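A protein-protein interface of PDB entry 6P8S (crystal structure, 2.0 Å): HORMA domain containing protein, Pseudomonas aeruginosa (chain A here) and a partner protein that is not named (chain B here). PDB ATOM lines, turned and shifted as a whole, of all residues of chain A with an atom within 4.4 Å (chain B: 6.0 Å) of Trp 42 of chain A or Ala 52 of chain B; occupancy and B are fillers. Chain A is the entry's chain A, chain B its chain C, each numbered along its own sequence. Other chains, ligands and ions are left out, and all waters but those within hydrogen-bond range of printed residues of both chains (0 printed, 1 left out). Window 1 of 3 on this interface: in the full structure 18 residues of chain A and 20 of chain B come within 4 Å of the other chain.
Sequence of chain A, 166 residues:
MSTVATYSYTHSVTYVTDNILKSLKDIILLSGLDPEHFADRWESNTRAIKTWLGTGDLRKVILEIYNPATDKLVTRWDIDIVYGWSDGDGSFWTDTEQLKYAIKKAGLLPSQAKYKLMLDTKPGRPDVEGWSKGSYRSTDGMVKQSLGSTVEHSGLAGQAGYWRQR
OD1 of Asp 18 of chain A sits at hydrogen-bond distance from N of Ala 17 of chain B (3.0 Å). The side-chain amino group (NZ) of Lys 22 of chain A lies within salt-bridge range of the side-chain carboxylate (OD1) of Asp 53 of chain B, 2.9 Å away.
OG1 of Thr 46 of chain A lies within hydrogen-bond range of O of Trp 42 of chain A, 2.9 Å away.
CA of Gly 45 of chain B touches O of Ala 39 of chain A, at 3.2 Å. Val 46 of chain B touches Ala 39 of chain A (N to CB, 3.8 Å). Gly 45 of chain B touches Trp 42 of chain A. Ala 48 of chain B touches Trp 42 of chain A (CB to NE1, 3.5 Å). CZ3 of Trp 42 of chain A touches OG of Ser 49 of chain B, at 3.6 Å. CZ2 of Trp 42 of chain A touches CB of Ala 52 of chain B (3.7 Å). Glu 43 of chain A touches Leu 18 of chain B (CG to CD2, 3.6 Å).
Trp 42 of chain A touches just these residues of chain B: Gly 45, Ala 48, Ser 49 and Ala 52. Printed residues of chain A within 4 Å of Ala 52 of chain B: Trp 42 (3.7 Å). Of the printed residues of chain B, Glu 43 of chain A touches Leu 18. Printed residues of chain B within 4 Å of Lys 22 of chain A: Asp 53. Printed residues of chain A within 4 Å of Ala 17 of chain B: Asp 18 (3.0 Å). Of the printed residues of chain B, Ala 39 of chain A touches Gly 45 (3.2 Å) and Val 46 (3.8 Å). Thr 44 of chain B touches none of the printed residues of chain A. Phe 38 of chain A touches none of the printed residues of chain B. The nearest printed residue of chain A that does not touch Ala 52 of chain B is Lys 22 of chain A (4.01 Å). The nearest printed residue of chain A that does not touch Ala 17 of chain B is Trp 42 of chain A (4.2 Å).
Of the 12 printed residues of chain A, 5 touch a printed residue of chain B. Printed residues of chain A that touch a printed residue of chain B: Asp 18, Lys 22, Ala 39, Trp 42 and Glu 43. Hydrophobic or aromatic side chains of chain A within 4 Å of the printed part of chain B: Ala 39 and Trp 42. Hydrophobic or aromatic side chains of chain B that line the printed part of chain A: Ala 17, Leu 18, Ala 48 and Ala 52. Among the printed residues, 9 pairs touch across the chains. Among the printed residues, Asp or Glu carboxylates within 4 Å of a Lys or Arg side-chain nitrogen of the other chain: Lys 22 of chain A with Asp 53 of chain B.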
ATOM      1  N   ASP A  18      20.998 -20.000 -22.421  1.00  0.00           N
ATOM      2  CA  ASP A  18      21.192 -20.240 -20.996  1.00  0.00           C
ATOM      3  C   ASP A  18      20.366 -19.275 -20.145  1.00  0.00           C
ATOM      4  O   ASP A  18      19.810 -19.663 -19.107  1.00  0.00           O
ATOM      5  CB  ASP A  18      22.673 -20.104 -20.639  1.00  0.00           C
ATOM      6  CG  ASP A  18      23.502 -21.313 -21.068  1.00  0.00           C
ATOM      7  OD1 ASP A  18      22.948 -22.435 -21.100  1.00  0.00           O
ATOM      8  OD2 ASP A  18      24.713 -21.140 -21.360  1.00  0.00           O
ATOM      9  N   LEU A  21      16.576 -19.809 -20.126  1.00  0.00           N
ATOM     10  CA  LEU A  21      16.244 -20.916 -19.230  1.00  0.00           C
ATOM     11  C   LEU A  21      16.488 -20.533 -17.771  1.00  0.00           C
ATOM     12  O   LEU A  21      15.687 -20.888 -16.891  1.00  0.00           O
ATOM     13  CB  LEU A  21      17.032 -22.169 -19.600  1.00  0.00           C
ATOM     14  CG  LEU A  21      16.614 -22.876 -20.889  1.00  0.00           C
ATOM     15  CD1 LEU A  21      17.430 -24.142 -21.108  1.00  0.00           C
ATOM     16  CD2 LEU A  21      15.115 -23.223 -20.910  1.00  0.00           C
ATOM     17  N   LYS A  22      17.582 -19.811 -17.492  1.00  0.00           N
ATOM     18  CA  LYS A  22      17.792 -19.281 -16.145  1.00  0.00           C
ATOM     19  C   LYS A  22      16.608 -18.423 -15.714  1.00  0.00           C
ATOM     20  O   LYS A  22      16.088 -18.570 -14.602  1.00  0.00           O
ATOM     21  CB  LYS A  22      19.095 -18.474 -16.086  1.00  0.00           C
ATOM     22  CG  LYS A  22      19.486 -17.961 -14.694  1.00  0.00           C
ATOM     23  CD  LYS A  22      19.306 -16.451 -14.575  1.00  0.00           C
ATOM     24  CE  LYS A  22      19.924 -15.879 -13.292  1.00  0.00           C
ATOM     25  NZ  LYS A  22      19.393 -16.513 -12.049  1.00  0.00           N
ATOM     26  N   PHE A  38      11.253 -28.537 -14.516  1.00  0.00           N
ATOM     27  CA  PHE A  38      12.036 -27.723 -15.441  1.00  0.00           C
ATOM     28  C   PHE A  38      13.455 -28.257 -15.569  1.00  0.00           C
ATOM     29  O   PHE A  38      14.049 -28.205 -16.656  1.00  0.00           O
ATOM     30  CB  PHE A  38      12.036 -26.267 -14.966  1.00  0.00           C
ATOM     31  CG  PHE A  38      12.414 -25.284 -16.029  1.00  0.00           C
ATOM     32  CD1 PHE A  38      11.568 -25.028 -17.088  1.00  0.00           C
ATOM     33  CD2 PHE A  38      13.612 -24.597 -15.956  1.00  0.00           C
ATOM     34  CE1 PHE A  38      11.920 -24.125 -18.070  1.00  0.00           C
ATOM     35  CE2 PHE A  38      13.964 -23.690 -16.929  1.00  0.00           C
ATOM     36  CZ  PHE A  38      13.112 -23.458 -17.990  1.00  0.00           C
ATOM     37  N   ALA A  39      14.010 -28.789 -14.479  1.00  0.00           N
ATOM     38  CA  ALA A  39      15.342 -29.368 -14.552  1.00  0.00           C
ATOM     39  C   ALA A  39      15.328 -30.651 -15.371  1.00  0.00           C
ATOM     40  O   ALA A  39      16.221 -30.878 -16.198  1.00  0.00           O
ATOM     41  CB  ALA A  39      15.874 -29.626 -13.143  1.00  0.00           C
ATOM     42  N   ASP A  40      14.311 -31.497 -15.162  1.00  0.00           N
ATOM     43  CA  ASP A  40      14.176 -32.719 -15.951  1.00  0.00           C
ATOM     44  C   ASP A  40      14.150 -32.439 -17.448  1.00  0.00           C
ATOM     45  O   ASP A  40      14.571 -33.285 -18.243  1.00  0.00           O
ATOM     46  CB  ASP A  40      12.902 -33.463 -15.563  1.00  0.00           C
ATOM     47  CG  ASP A  40      12.971 -34.070 -14.183  1.00  0.00           C
ATOM     48  OD1 ASP A  40      14.092 -34.346 -13.708  1.00  0.00           O
ATOM     49  OD2 ASP A  40      11.896 -34.278 -13.571  1.00  0.00           O
ATOM     50  N   ARG A  41      13.677 -31.266 -17.856  1.00  0.00           N
ATOM     51  CA  ARG A  41      13.583 -30.924 -19.268  1.00  0.00           C
ATOM     52  C   ARG A  41      14.707 -30.005 -19.747  1.00  0.00           C
ATOM     53  O   ARG A  41      14.720 -29.615 -20.923  1.00  0.00           O
ATOM     54  CB  ARG A  41      12.234 -30.264 -19.555  1.00  0.00           C
ATOM     55  CG  ARG A  41      11.023 -31.160 -19.316  1.00  0.00           C
ATOM     56  CD  ARG A  41      10.957 -32.318 -20.313  1.00  0.00           C
ATOM     57  NE  ARG A  41       9.765 -33.138 -20.116  1.00  0.00           N
ATOM     58  CZ  ARG A  41       8.570 -32.863 -20.638  1.00  0.00           C
ATOM     59  NH1 ARG A  41       8.401 -31.788 -21.397  1.00  0.00           N
ATOM     60  NH2 ARG A  41       7.539 -33.668 -20.406  1.00  0.00           N
ATOM     61  N   TRP A  42      15.652 -29.656 -18.872  1.00  0.00           N
ATOM     62  CA  TRP A  42      16.677 -28.683 -19.239  1.00  0.00           C
ATOM     63  C   TRP A  42      17.411 -29.105 -20.503  1.00  0.00           C
ATOM     64  O   TRP A  42      17.606 -28.294 -21.419  1.00  0.00           O
ATOM     65  CB  TRP A  42      17.658 -28.505 -18.079  1.00  0.00           C
ATOM     66  CG  TRP A  42      18.555 -27.312 -18.235  1.00  0.00           C
ATOM     67  CD1 TRP A  42      19.669 -27.219 -19.016  1.00  0.00           C
ATOM     68  CD2 TRP A  42      18.409 -26.037 -17.582  1.00  0.00           C
ATOM     69  NE1 TRP A  42      20.226 -25.969 -18.894  1.00  0.00           N
ATOM     70  CE2 TRP A  42      19.469 -25.222 -18.025  1.00  0.00           C
ATOM     71  CE3 TRP A  42      17.492 -25.516 -16.666  1.00  0.00           C
ATOM     72  CZ2 TRP A  42      19.633 -23.915 -17.586  1.00  0.00           C
ATOM     73  CZ3 TRP A  42      17.655 -24.218 -16.230  1.00  0.00           C
ATOM     74  CH2 TRP A  42      18.719 -23.429 -16.690  1.00  0.00           C
ATOM     75  N   GLU A  43      17.826 -30.372 -20.572  1.00  0.00           N
ATOM     76  CA  GLU A  43      18.584 -30.848 -21.726  1.00  0.00           C
ATOM     77  C   GLU A  43      17.763 -30.716 -23.003  1.00  0.00           C
ATOM     78  O   GLU A  43      18.204 -30.093 -23.975  1.00  0.00           O
ATOM     79  CB  GLU A  43      19.016 -32.298 -21.493  1.00  0.00           C
ATOM     80  CG  GLU A  43      19.737 -32.935 -22.654  1.00  0.00           C
ATOM     81  CD  GLU A  43      20.201 -34.346 -22.335  1.00  0.00           C
ATOM     82  OE1 GLU A  43      19.350 -35.212 -22.012  1.00  0.00           O
ATOM     83  OE2 GLU A  43      21.423 -34.595 -22.386  1.00  0.00           O
ATOM     84  N   SER A  44      16.556 -31.287 -23.014  1.00  0.00           N
ATOM     85  CA  SER A  44      15.682 -31.159 -24.179  1.00  0.00           C
ATOM     86  C   SER A  44      15.420 -29.693 -24.520  1.00  0.00           C
ATOM     87  O   SER A  44      15.494 -29.290 -25.687  1.00  0.00           O
ATOM     88  CB  SER A  44      14.358 -31.881 -23.920  1.00  0.00           C
ATOM     89  OG  SER A  44      14.565 -33.177 -23.390  1.00  0.00           O
ATOM     90  N   ASN A  45      15.096 -28.880 -23.514  1.00  0.00           N
ATOM     91  CA  ASN A  45      14.798 -27.474 -23.776  1.00  0.00           C
ATOM     92  C   ASN A  45      16.012 -26.745 -24.339  1.00  0.00           C
ATOM     93  O   ASN A  45      15.883 -25.944 -25.275  1.00  0.00           O
ATOM     94  CB  ASN A  45      14.301 -26.798 -22.496  1.00  0.00           C
ATOM     95  CG  ASN A  45      12.938 -27.310 -22.067  1.00  0.00           C
ATOM     96  OD1 ASN A  45      12.238 -27.964 -22.840  1.00  0.00           O
ATOM     97  ND2 ASN A  45      12.551 -27.006 -20.832  1.00  0.00           N
ATOM     98  N   THR A  46      17.200 -27.001 -23.775  1.00  0.00           N
ATOM     99  CA  THR A  46      18.415 -26.379 -24.292  1.00  0.00           C
ATOM    100  C   THR A  46      18.603 -26.698 -25.772  1.00  0.00           C
ATOM    101  O   THR A  46      18.728 -25.797 -26.604  1.00  0.00           O
ATOM    102  CB  THR A  46      19.628 -26.852 -23.488  1.00  0.00           C
ATOM    103  OG1 THR A  46      19.558 -26.338 -22.153  1.00  0.00           O
ATOM    104  CG2 THR A  46      20.928 -26.394 -24.150  1.00  0.00           C
ATOM    105  N   ALA B  17      25.176 -24.342 -20.506  1.00  0.00           N
ATOM    106  CA  ALA B  17      25.224 -24.955 -19.183  1.00  0.00           C
ATOM    107  C   ALA B  17      25.143 -26.472 -19.272  1.00  0.00           C
ATOM    108  O   ALA B  17      25.834 -27.180 -18.524  1.00  0.00           O
ATOM    109  CB  ALA B  17      24.097 -24.398 -18.302  1.00  0.00           C
ATOM    110  N   LEU B  18      24.313 -26.990 -20.181  1.00  0.00           N
ATOM    111  CA  LEU B  18      24.242 -28.434 -20.393  1.00  0.00           C
ATOM    112  C   LEU B  18      25.592 -28.984 -20.835  1.00  0.00           C
ATOM    113  O   LEU B  18      26.095 -29.971 -20.284  1.00  0.00           O
ATOM    114  CB  LEU B  18      23.180 -28.751 -21.439  1.00  0.00           C
ATOM    115  CG  LEU B  18      23.071 -30.201 -21.889  1.00  0.00           C
ATOM    116  CD1 LEU B  18      22.580 -31.101 -20.789  1.00  0.00           C
ATOM    117  CD2 LEU B  18      22.157 -30.281 -23.120  1.00  0.00           C
ATOM    118  N   THR B  44      21.728 -34.087 -14.336  1.00  0.00           N
ATOM    119  CA  THR B  44      22.173 -33.124 -15.330  1.00  0.00           C
ATOM    120  C   THR B  44      21.377 -31.834 -15.236  1.00  0.00           C
ATOM    121  O   THR B  44      21.960 -30.745 -15.213  1.00  0.00           O
ATOM    122  CB  THR B  44      22.046 -33.744 -16.722  1.00  0.00           C
ATOM    123  OG1 THR B  44      23.067 -34.736 -16.891  1.00  0.00           O
ATOM    124  CG2 THR B  44      22.182 -32.689 -17.797  1.00  0.00           C
ATOM    125  N   GLY B  45      20.043 -31.932 -15.183  1.00  0.00           N
ATOM    126  CA  GLY B  45      19.228 -30.730 -15.221  1.00  0.00           C
ATOM    127  C   GLY B  45      19.460 -29.821 -14.028  1.00  0.00           C
ATOM    128  O   GLY B  45      19.513 -28.598 -14.169  1.00  0.00           O
ATOM    129  N   VAL B  46      19.581 -30.406 -12.838  1.00  0.00           N
ATOM    130  CA  VAL B  46      19.866 -29.626 -11.640  1.00  0.00           C
ATOM    131  C   VAL B  46      21.226 -28.944 -11.758  1.00  0.00           C
ATOM    132  O   VAL B  46      21.378 -27.754 -11.449  1.00  0.00           O
ATOM    133  CB  VAL B  46      19.792 -30.530 -10.397  1.00  0.00           C
ATOM    134  CG1 VAL B  46      20.114 -29.737  -9.147  1.00  0.00           C
ATOM    135  CG2 VAL B  46      18.405 -31.172 -10.295  1.00  0.00           C
ATOM    136  N   ALA B  47      22.243 -29.689 -12.196  1.00  0.00           N
ATOM    137  CA  ALA B  47      23.587 -29.120 -12.260  1.00  0.00           C
ATOM    138  C   ALA B  47      23.668 -28.017 -13.309  1.00  0.00           C
ATOM    139  O   ALA B  47      24.289 -26.974 -13.072  1.00  0.00           O
ATOM    140  CB  ALA B  47      24.611 -30.220 -12.555  1.00  0.00           C
ATOM    141  N   ALA B  48      23.041 -28.232 -14.476  1.00  0.00           N
ATOM    142  CA  ALA B  48      23.035 -27.212 -15.522  1.00  0.00           C
ATOM    143  C   ALA B  48      22.334 -25.950 -15.045  1.00  0.00           C
ATOM    144  O   ALA B  48      22.782 -24.832 -15.328  1.00  0.00           O
ATOM    145  CB  ALA B  48      22.359 -27.755 -16.784  1.00  0.00           C
ATOM    146  N   SER B  49      21.220 -26.104 -14.332  1.00  0.00           N
ATOM    147  CA  SER B  49      20.521 -24.932 -13.807  1.00  0.00           C
ATOM    148  C   SER B  49      21.431 -24.120 -12.890  1.00  0.00           C
ATOM    149  O   SER B  49      21.446 -22.883 -12.950  1.00  0.00           O
ATOM    150  CB  SER B  49      19.253 -25.366 -13.071  1.00  0.00           C
ATOM    151  OG  SER B  49      18.453 -24.251 -12.686  1.00  0.00           O
ATOM    152  N   LEU B  50      22.209 -24.805 -12.044  1.00  0.00           N
ATOM    153  CA  LEU B  50      23.128 -24.115 -11.146  1.00  0.00           C
ATOM    154  C   LEU B  50      24.241 -23.434 -11.923  1.00  0.00           C
ATOM    155  O   LEU B  50      24.647 -22.316 -11.588  1.00  0.00           O
ATOM    156  CB  LEU B  50      23.706 -25.100 -10.136  1.00  0.00           C
ATOM    157  CG  LEU B  50      22.743 -25.541  -9.029  1.00  0.00           C
ATOM    158  CD1 LEU B  50      23.325 -26.682  -8.230  1.00  0.00           C
ATOM    159  CD2 LEU B  50      22.425 -24.360  -8.132  1.00  0.00           C
ATOM    160  N   ILE B  51      24.759 -24.104 -12.950  1.00  0.00           N
ATOM    161  CA  ILE B  51      25.781 -23.510 -13.801  1.00  0.00           C
ATOM    162  C   ILE B  51      25.246 -22.266 -14.482  1.00  0.00           C
ATOM    163  O   ILE B  51      25.933 -21.239 -14.553  1.00  0.00           O
ATOM    164  CB  ILE B  51      26.283 -24.546 -14.826  1.00  0.00           C
ATOM    165  CG1 ILE B  51      27.167 -25.577 -14.134  1.00  0.00           C
ATOM    166  CG2 ILE B  51      26.992 -23.846 -15.963  1.00  0.00           C
ATOM    167  CD1 ILE B  51      27.321 -26.836 -14.938  1.00  0.00           C
ATOM    168  N   ALA B  52      24.017 -22.333 -15.004  1.00  0.00           N
ATOM    169  CA  ALA B  52      23.404 -21.150 -15.594  1.00  0.00           C
ATOM    170  C   ALA B  52      23.286 -20.027 -14.574  1.00  0.00           C
ATOM    171  O   ALA B  52      23.389 -18.849 -14.936  1.00  0.00           O
ATOM    172  CB  ALA B  52      22.031 -21.504 -16.165  1.00  0.00           C
ATOM    173  N   ASP B  53      23.060 -20.371 -13.301  1.00  0.00           N
ATOM    174  CA  ASP B  53      23.099 -19.397 -12.216  1.00  0.00           C
ATOM    175  C   ASP B  53      24.515 -18.928 -11.886  1.00  0.00           C
ATOM    176  O   ASP B  53      24.683 -18.089 -10.991  1.00  0.00           O
ATOM    177  CB  ASP B  53      22.467 -19.990 -10.956  1.00  0.00           C
ATOM    178  CG  ASP B  53      20.957 -20.109 -11.053  1.00  0.00           C
ATOM    179  OD1 ASP B  53      20.326 -19.269 -11.749  1.00  0.00           O
ATOM    180  OD2 ASP B  53      20.397 -21.041 -10.425  1.00  0.00           O
ATOM    181  N   GLN B  54      25.526 -19.455 -12.570  1.00  0.00           N
ATOM    182  CA  GLN B  54      26.928 -19.161 -12.302  1.00  0.00           C
ATOM    183  C   GLN B  54      27.336 -19.551 -10.889  1.00  0.00           C
ATOM    184  O   GLN B  54      28.281 -18.972 -10.328  1.00  0.00           O
ATOM    185  CB  GLN B  54      27.242 -17.679 -12.544  1.00  0.00           C
ATOM    186  CG  GLN B  54      27.079 -17.258 -13.994  1.00  0.00           C
ATOM    187  CD  GLN B  54      27.595 -15.873 -14.257  1.00  0.00           C
ATOM    188  OE1 GLN B  54      28.172 -15.244 -13.377  1.00  0.00           O
ATOM    189  NE2 GLN B  54      27.381 -15.379 -15.466  1.00  0.00           N
ATOM    190  N   ALA B  55      26.636 -20.515 -10.298  1.00  0.00           N
ATOM    191  CA  ALA B  55      26.998 -20.969  -8.962  1.00  0.00           C
ATOM    192  C   ALA B  55      28.455 -21.408  -8.863  1.00  0.00           C
ATOM    193  O   ALA B  55      29.076 -21.152  -7.816  1.00  0.00           O
ATOM    194  CB  ALA B  55      26.069 -22.110  -8.536  1.00  0.00           C
ATOM    195  N   PRO B  56      29.057 -22.054  -9.870  1.00  0.00           N
ATOM    196  CA  PRO B  56      30.460 -22.475  -9.723  1.00  0.00           C
ATOM    197  C   PRO B  56      31.483 -21.424 -10.125  1.00  0.00           C
ATOM    198  O   PRO B  56      32.648 -21.765 -10.344  1.00  0.00           O
ATOM    199  CB  PRO B  56      30.569 -23.706 -10.646  1.00  0.00           C
ATOM    200  CG  PRO B  56      29.137 -24.074 -11.039  1.00  0.00           C
ATOM    201  CD  PRO B  56      28.379 -22.758 -10.978  1.00  0.00           C
ATOM    202  N   PHE B  76      32.936 -17.668 -17.198  1.00  0.00           N
ATOM    203  CA  PHE B  76      31.781 -17.192 -17.945  1.00  0.00           C
ATOM    204  C   PHE B  76      32.146 -15.930 -18.710  1.00  0.00           C
ATOM    205  O   PHE B  76      33.118 -15.241 -18.391  1.00  0.00           O
ATOM    206  CB  PHE B  76      30.580 -16.903 -17.024  1.00  0.00           C
ATOM    207  CG  PHE B  76      30.093 -18.102 -16.262  1.00  0.00           C
ATOM    208  CD1 PHE B  76      29.139 -18.944 -16.806  1.00  0.00           C
ATOM    209  CD2 PHE B  76      30.582 -18.382 -15.004  1.00  0.00           C
ATOM    210  CE1 PHE B  76      28.691 -20.056 -16.111  1.00  0.00           C
ATOM    211  CE2 PHE B  76      30.140 -19.485 -14.297  1.00  0.00           C
ATOM    212  CZ  PHE B  76      29.196 -20.327 -14.851  1.00  0.00           C
